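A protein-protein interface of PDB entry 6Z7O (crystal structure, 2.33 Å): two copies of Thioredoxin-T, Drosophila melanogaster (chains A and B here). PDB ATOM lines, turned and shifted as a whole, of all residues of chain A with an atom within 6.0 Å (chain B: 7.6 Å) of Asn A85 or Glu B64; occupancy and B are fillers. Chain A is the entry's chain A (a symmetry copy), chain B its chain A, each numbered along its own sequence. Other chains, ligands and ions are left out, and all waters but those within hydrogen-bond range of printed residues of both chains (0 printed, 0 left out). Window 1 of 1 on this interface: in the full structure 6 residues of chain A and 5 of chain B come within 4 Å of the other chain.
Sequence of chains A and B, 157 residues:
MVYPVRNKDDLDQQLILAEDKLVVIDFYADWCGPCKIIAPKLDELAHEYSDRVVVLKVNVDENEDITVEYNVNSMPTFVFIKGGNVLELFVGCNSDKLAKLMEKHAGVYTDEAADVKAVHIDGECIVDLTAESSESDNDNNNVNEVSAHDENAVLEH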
ATOM      1  N   PHE A  80     -20.750   7.274   9.430  1.00  0.00           N
ATOM      2  CA  PHE A  80     -20.505   8.715   9.432  1.00  0.00           C
ATOM      3  C   PHE A  80     -19.651   9.102   8.221  1.00  0.00           C
ATOM      4  O   PHE A  80     -18.523   8.614   8.075  1.00  0.00           O
ATOM      5  CB  PHE A  80     -19.807   9.135  10.728  1.00  0.00           C
ATOM      6  CG  PHE A  80     -20.685   9.043  11.932  1.00  0.00           C
ATOM      7  CD1 PHE A  80     -21.046   7.812  12.442  1.00  0.00           C
ATOM      8  CD2 PHE A  80     -21.170  10.189  12.549  1.00  0.00           C
ATOM      9  CE1 PHE A  80     -21.865   7.725  13.552  1.00  0.00           C
ATOM     10  CE2 PHE A  80     -21.986  10.102  13.653  1.00  0.00           C
ATOM     11  CZ  PHE A  80     -22.339   8.872  14.157  1.00  0.00           C
ATOM     12  N   ILE A  81     -20.175  10.007   7.379  1.00  0.00           N
ATOM     13  CA  ILE A  81     -19.573  10.338   6.089  1.00  0.00           C
ATOM     14  C   ILE A  81     -19.438  11.845   5.966  1.00  0.00           C
ATOM     15  O   ILE A  81     -20.299  12.601   6.435  1.00  0.00           O
ATOM     16  CB  ILE A  81     -20.401   9.779   4.908  1.00  0.00           C
ATOM     17  CG1 ILE A  81     -20.215   8.270   4.790  1.00  0.00           C
ATOM     18  CG2 ILE A  81     -20.000  10.405   3.590  1.00  0.00           C
ATOM     19  CD1 ILE A  81     -21.377   7.585   4.085  1.00  0.00           C
ATOM     20  N   LYS A  82     -18.341  12.286   5.360  1.00  0.00           N
ATOM     21  CA  LYS A  82     -18.142  13.691   5.031  1.00  0.00           C
ATOM     22  C   LYS A  82     -17.380  13.767   3.720  1.00  0.00           C
ATOM     23  O   LYS A  82     -16.264  13.243   3.624  1.00  0.00           O
ATOM     24  CB  LYS A  82     -17.407  14.444   6.144  1.00  0.00           C
ATOM     25  CG  LYS A  82     -17.235  15.937   5.885  1.00  0.00           C
ATOM     26  CD  LYS A  82     -16.021  16.484   6.658  1.00  0.00           C
ATOM     27  CE  LYS A  82     -15.770  17.965   6.336  1.00  0.00           C
ATOM     28  NZ  LYS A  82     -16.338  18.915   7.355  1.00  0.00           N
ATOM     29  N   GLY A  83     -17.991  14.317   2.670  1.00  0.00           N
ATOM     30  CA  GLY A  83     -17.390  14.413   1.361  1.00  0.00           C
ATOM     31  C   GLY A  83     -17.335  13.128   0.581  1.00  0.00           C
ATOM     32  O   GLY A  83     -16.410  12.949  -0.206  1.00  0.00           O
ATOM     33  N   GLY A  84     -18.293  12.221   0.764  1.00  0.00           N
ATOM     34  CA  GLY A  84     -18.167  10.906   0.165  1.00  0.00           C
ATOM     35  C   GLY A  84     -17.168   9.991   0.836  1.00  0.00           C
ATOM     36  O   GLY A  84     -17.086   8.817   0.454  1.00  0.00           O
ATOM     37  N   ASN A  85     -16.424  10.490   1.832  1.00  0.00           N
ATOM     38  CA  ASN A  85     -15.501   9.651   2.581  1.00  0.00           C
ATOM     39  C   ASN A  85     -16.164   9.102   3.835  1.00  0.00           C
ATOM     40  O   ASN A  85     -16.702   9.872   4.641  1.00  0.00           O
ATOM     41  CB  ASN A  85     -14.280  10.462   3.015  1.00  0.00           C
ATOM     42  CG  ASN A  85     -13.127  10.318   2.081  1.00  0.00           C
ATOM     43  OD1 ASN A  85     -13.251   9.708   1.017  1.00  0.00           O
ATOM     44  ND2 ASN A  85     -11.986  10.900   2.455  1.00  0.00           N
ATOM     45  N   VAL A  86     -15.975   7.800   4.039  1.00  0.00           N
ATOM     46  CA  VAL A  86     -16.411   7.157   5.277  1.00  0.00           C
ATOM     47  C   VAL A  86     -15.391   7.497   6.356  1.00  0.00           C
ATOM     48  O   VAL A  86     -14.256   7.022   6.309  1.00  0.00           O
ATOM     49  CB  VAL A  86     -16.554   5.639   5.115  1.00  0.00           C
ATOM     50  CG1 VAL A  86     -16.767   5.004   6.467  1.00  0.00           C
ATOM     51  CG2 VAL A  86     -17.707   5.309   4.186  1.00  0.00           C
ATOM     52  N   LEU A  87     -15.786   8.325   7.330  1.00  0.00           N
ATOM     53  CA  LEU A  87     -14.896   8.614   8.456  1.00  0.00           C
ATOM     54  C   LEU A  87     -14.864   7.470   9.471  1.00  0.00           C
ATOM     55  O   LEU A  87     -13.782   7.030   9.882  1.00  0.00           O
ATOM     56  CB  LEU A  87     -15.327   9.902   9.150  1.00  0.00           C
ATOM     57  CG  LEU A  87     -15.637  11.113   8.280  1.00  0.00           C
ATOM     58  CD1 LEU A  87     -16.223  12.185   9.138  1.00  0.00           C
ATOM     59  CD2 LEU A  87     -14.370  11.602   7.595  1.00  0.00           C
ATOM     60  N   VAL B  58       0.026  14.068  12.748  1.00  0.00           N
ATOM     61  CA  VAL B  58      -1.103  13.492  12.034  1.00  0.00           C
ATOM     62  C   VAL B  58      -1.036  13.958  10.585  1.00  0.00           C
ATOM     63  O   VAL B  58      -1.117  15.165  10.300  1.00  0.00           O
ATOM     64  CB  VAL B  58      -2.440  13.879  12.680  1.00  0.00           C
ATOM     65  CG1 VAL B  58      -3.610  13.641  11.698  1.00  0.00           C
ATOM     66  CG2 VAL B  58      -2.632  13.100  13.987  1.00  0.00           C
ATOM     67  N   ASN B  59      -0.882  13.001   9.679  1.00  0.00           N
ATOM     68  CA  ASN B  59      -0.889  13.266   8.249  1.00  0.00           C
ATOM     69  C   ASN B  59      -2.335  13.396   7.792  1.00  0.00           C
ATOM     70  O   ASN B  59      -3.090  12.425   7.830  1.00  0.00           O
ATOM     71  CB  ASN B  59      -0.168  12.137   7.510  1.00  0.00           C
ATOM     72  CG  ASN B  59      -0.013  12.418   6.030  1.00  0.00           C
ATOM     73  OD1 ASN B  59      -0.992  12.727   5.333  1.00  0.00           O
ATOM     74  ND2 ASN B  59       1.222  12.345   5.544  1.00  0.00           N
ATOM     75  N   VAL B  60      -2.725  14.591   7.347  1.00  0.00           N
ATOM     76  CA  VAL B  60      -4.146  14.834   7.111  1.00  0.00           C
ATOM     77  C   VAL B  60      -4.649  14.037   5.907  1.00  0.00           C
ATOM     78  O   VAL B  60      -5.828  13.670   5.847  1.00  0.00           O
ATOM     79  CB  VAL B  60      -4.434  16.342   6.945  1.00  0.00           C
ATOM     80  CG1 VAL B  60      -3.998  17.135   8.187  1.00  0.00           C
ATOM     81  CG2 VAL B  60      -3.779  16.876   5.690  1.00  0.00           C
ATOM     82  N   ASP B  61      -3.781  13.752   4.934  1.00  0.00           N
ATOM     83  CA  ASP B  61      -4.231  13.010   3.763  1.00  0.00           C
ATOM     84  C   ASP B  61      -4.590  11.575   4.092  1.00  0.00           C
ATOM     85  O   ASP B  61      -5.398  10.979   3.385  1.00  0.00           O
ATOM     86  CB  ASP B  61      -3.165  13.027   2.674  1.00  0.00           C
ATOM     87  CG  ASP B  61      -3.063  14.362   1.999  1.00  0.00           C
ATOM     88  OD1 ASP B  61      -4.105  15.022   1.835  1.00  0.00           O
ATOM     89  OD2 ASP B  61      -1.941  14.758   1.640  1.00  0.00           O
ATOM     90  N   GLU B  62      -4.026  11.012   5.145  1.00  0.00           N
ATOM     91  CA  GLU B  62      -4.460   9.662   5.458  1.00  0.00           C
ATOM     92  C   GLU B  62      -5.324   9.588   6.710  1.00  0.00           C
ATOM     93  O   GLU B  62      -5.810   8.503   7.053  1.00  0.00           O
ATOM     94  CB  GLU B  62      -3.232   8.757   5.599  1.00  0.00           C
ATOM     95  CG  GLU B  62      -2.973   7.880   4.378  1.00  0.00           C
ATOM     96  CD  GLU B  62      -1.523   7.437   4.289  1.00  0.00           C
ATOM     97  OE1 GLU B  62      -0.744   7.732   5.224  1.00  0.00           O
ATOM     98  OE2 GLU B  62      -1.166   6.785   3.282  1.00  0.00           O
ATOM     99  N   ASN B  63      -5.741  10.729   7.248  1.00  0.00           N
ATOM    100  CA  ASN B  63      -6.456  10.756   8.513  1.00  0.00           C
ATOM    101  C   ASN B  63      -7.557  11.809   8.457  1.00  0.00           C
ATOM    102  O   ASN B  63      -7.603  12.767   9.231  1.00  0.00           O
ATOM    103  CB  ASN B  63      -5.498  11.009   9.672  1.00  0.00           C
ATOM    104  CG  ASN B  63      -4.689   9.774  10.032  1.00  0.00           C
ATOM    105  OD1 ASN B  63      -5.206   8.809  10.624  1.00  0.00           O
ATOM    106  ND2 ASN B  63      -3.422   9.791   9.666  1.00  0.00           N
ATOM    107  N   GLU B  64      -8.473  11.604   7.517  1.00  0.00           N
ATOM    108  CA  GLU B  64      -9.640  12.466   7.422  1.00  0.00           C
ATOM    109  C   GLU B  64     -10.481  12.421   8.691  1.00  0.00           C
ATOM    110  O   GLU B  64     -11.087  13.429   9.064  1.00  0.00           O
ATOM    111  CB  GLU B  64     -10.463  12.075   6.191  1.00  0.00           C
ATOM    112  CG  GLU B  64      -9.607  11.906   4.916  1.00  0.00           C
ATOM    113  CD  GLU B  64      -9.211  10.444   4.619  1.00  0.00           C
ATOM    114  OE1 GLU B  64      -8.725   9.717   5.531  1.00  0.00           O
ATOM    115  OE2 GLU B  64      -9.390  10.024   3.448  1.00  0.00           O
ATOM    116  N   ASP B  65     -10.520  11.278   9.380  1.00  0.00           N
ATOM    117  CA  ASP B  65     -11.352  11.187  10.571  1.00  0.00           C
ATOM    118  C   ASP B  65     -10.812  12.067  11.691  1.00  0.00           C
ATOM    119  O   ASP B  65     -11.559  12.850  12.291  1.00  0.00           O
ATOM    120  CB  ASP B  65     -11.466   9.746  11.045  1.00  0.00           C
ATOM    121  CG  ASP B  65     -12.377   9.628  12.242  1.00  0.00           C
ATOM    122  OD1 ASP B  65     -13.345  10.398  12.285  1.00  0.00           O
ATOM    123  OD2 ASP B  65     -12.108   8.827  13.161  1.00  0.00           O
ATOM    124  N   ILE B  66      -9.517  11.954  11.992  1.00  0.00           N
ATOM    125  CA  ILE B  66      -8.944  12.767  13.062  1.00  0.00           C
ATOM    126  C   ILE B  66      -9.028  14.253  12.731  1.00  0.00           C
ATOM    127  O   ILE B  66      -9.256  15.086  13.624  1.00  0.00           O
ATOM    128  CB  ILE B  66      -7.495  12.333  13.329  1.00  0.00           C
ATOM    129  CG1 ILE B  66      -7.482  10.869  13.764  1.00  0.00           C
ATOM    130  CG2 ILE B  66      -6.878  13.236  14.365  1.00  0.00           C
ATOM    131  CD1 ILE B  66      -6.117  10.338  14.137  1.00  0.00           C
ATOM    132  N   THR B  67      -8.863  14.613  11.451  1.00  0.00           N
ATOM    133  CA  THR B  67      -8.908  16.023  11.056  1.00  0.00           C
ATOM    134  C   THR B  67     -10.291  16.629  11.286  1.00  0.00           C
ATOM    135  O   THR B  67     -10.413  17.762  11.788  1.00  0.00           O
ATOM    136  CB  THR B  67      -8.477  16.163   9.589  1.00  0.00           C
ATOM    137  OG1 THR B  67      -7.078  15.873   9.478  1.00  0.00           O
ATOM    138  CG2 THR B  67      -8.714  17.565   9.073  1.00  0.00           C
ATOM    139  N   VAL B  68     -11.345  15.867  10.969  1.00  0.00           N
ATOM    140  CA  VAL B  68     -12.712  16.341  11.158  1.00  0.00           C
ATOM    141  C   VAL B  68     -13.025  16.504  12.647  1.00  0.00           C
ATOM    142  O   VAL B  68     -13.646  17.495  13.063  1.00  0.00           O
ATOM    143  CB  VAL B  68     -13.687  15.372  10.471  1.00  0.00           C
ATOM    144  CG1 VAL B  68     -15.092  15.526  11.036  1.00  0.00           C
ATOM    145  CG2 VAL B  68     -13.662  15.577   8.995  1.00  0.00           C
ATOM    146  N   GLU B  69     -12.589  15.541  13.468  1.00  0.00           N
ATOM    147  CA  GLU B  69     -12.839  15.595  14.903  1.00  0.00           C
ATOM    148  C   GLU B  69     -12.162  16.789  15.580  1.00  0.00           C
ATOM    149  O   GLU B  69     -12.670  17.293  16.582  1.00  0.00           O
ATOM    150  CB  GLU B  69     -12.370  14.304  15.557  1.00  0.00           C
ATOM    151  CG  GLU B  69     -13.155  13.079  15.146  1.00  0.00           C
ATOM    152  CD  GLU B  69     -12.873  11.868  16.031  1.00  0.00           C
ATOM    153  OE1 GLU B  69     -11.970  11.932  16.911  1.00  0.00           O
ATOM    154  OE2 GLU B  69     -13.553  10.844  15.830  1.00  0.00           O
ATOM    155  N   TYR B  70     -11.009  17.236  15.086  1.00  0.00           N
ATOM    156  CA  TYR B  70     -10.330  18.387  15.664  1.00  0.00           C
ATOM    157  C   TYR B  70     -10.622  19.676  14.909  1.00  0.00           C
ATOM    158  O   TYR B  70     -10.001  20.706  15.196  1.00  0.00           O
ATOM    159  CB  TYR B  70      -8.823  18.120  15.733  1.00  0.00           C
ATOM    160  CG  TYR B  70      -8.494  17.221  16.892  1.00  0.00           C
ATOM    161  CD1 TYR B  70      -8.648  15.837  16.782  1.00  0.00           C
ATOM    162  CD2 TYR B  70      -8.098  17.750  18.124  1.00  0.00           C
ATOM    163  CE1 TYR B  70      -8.383  14.992  17.850  1.00  0.00           C
ATOM    164  CE2 TYR B  70      -7.831  16.901  19.220  1.00  0.00           C
ATOM    165  CZ  TYR B  70      -7.976  15.518  19.065  1.00  0.00           C
ATOM    166  OH  TYR B  70      -7.707  14.656  20.108  1.00  0.00           O
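No position is printed for both chains.
Hydrophobic or aromatic side chains of chain A that line the printed part of chain B: Leu A87. Among the printed residues, no Asp or Glu carboxylate lies within 4 Å of a Lys or Arg side-chain nitrogen of the other chain.
Lys A82 touches Val B68 (CD to CG2, 3.4 Å). Leu A87 touches Asp B65 (CB to OD1, 3.7 Å).
Of the printed residues of chain B, Lys A82 touches Val B68. No residue of chain B comes within 4 Å of Gly A84. Asn A85 touches just one residue of chain B: Glu B64 (2.9 Å). Of the printed residues of chain B, Leu A87 touches Asp B65. Glu B64 touches just one residue of chain A: Asn A85 (2.9 Å). Printed residues of chain A within 4 Å of Asp B65: Leu A87 (3.7 Å). Of the printed residues of chain A, Val B68 touches Lys A82 (3.4 Å). The nearest residue of chain B that does not touch Asn A85 is Asp B61 (6.7 Å). The nearest residue of chain A that does not touch Glu B64 is Leu A87 (4.03 Å). The nearest printed residue of chain B that does not touch Leu A87 is Val B68 (4.01 Å).
OE2 of Glu B64 lies within hydrogen-bond range of ND2 of Asn A85 (2.9 Å).
O of Phe A80 is in hydrogen-bond range of N of Leu A87 (2.9 Å).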
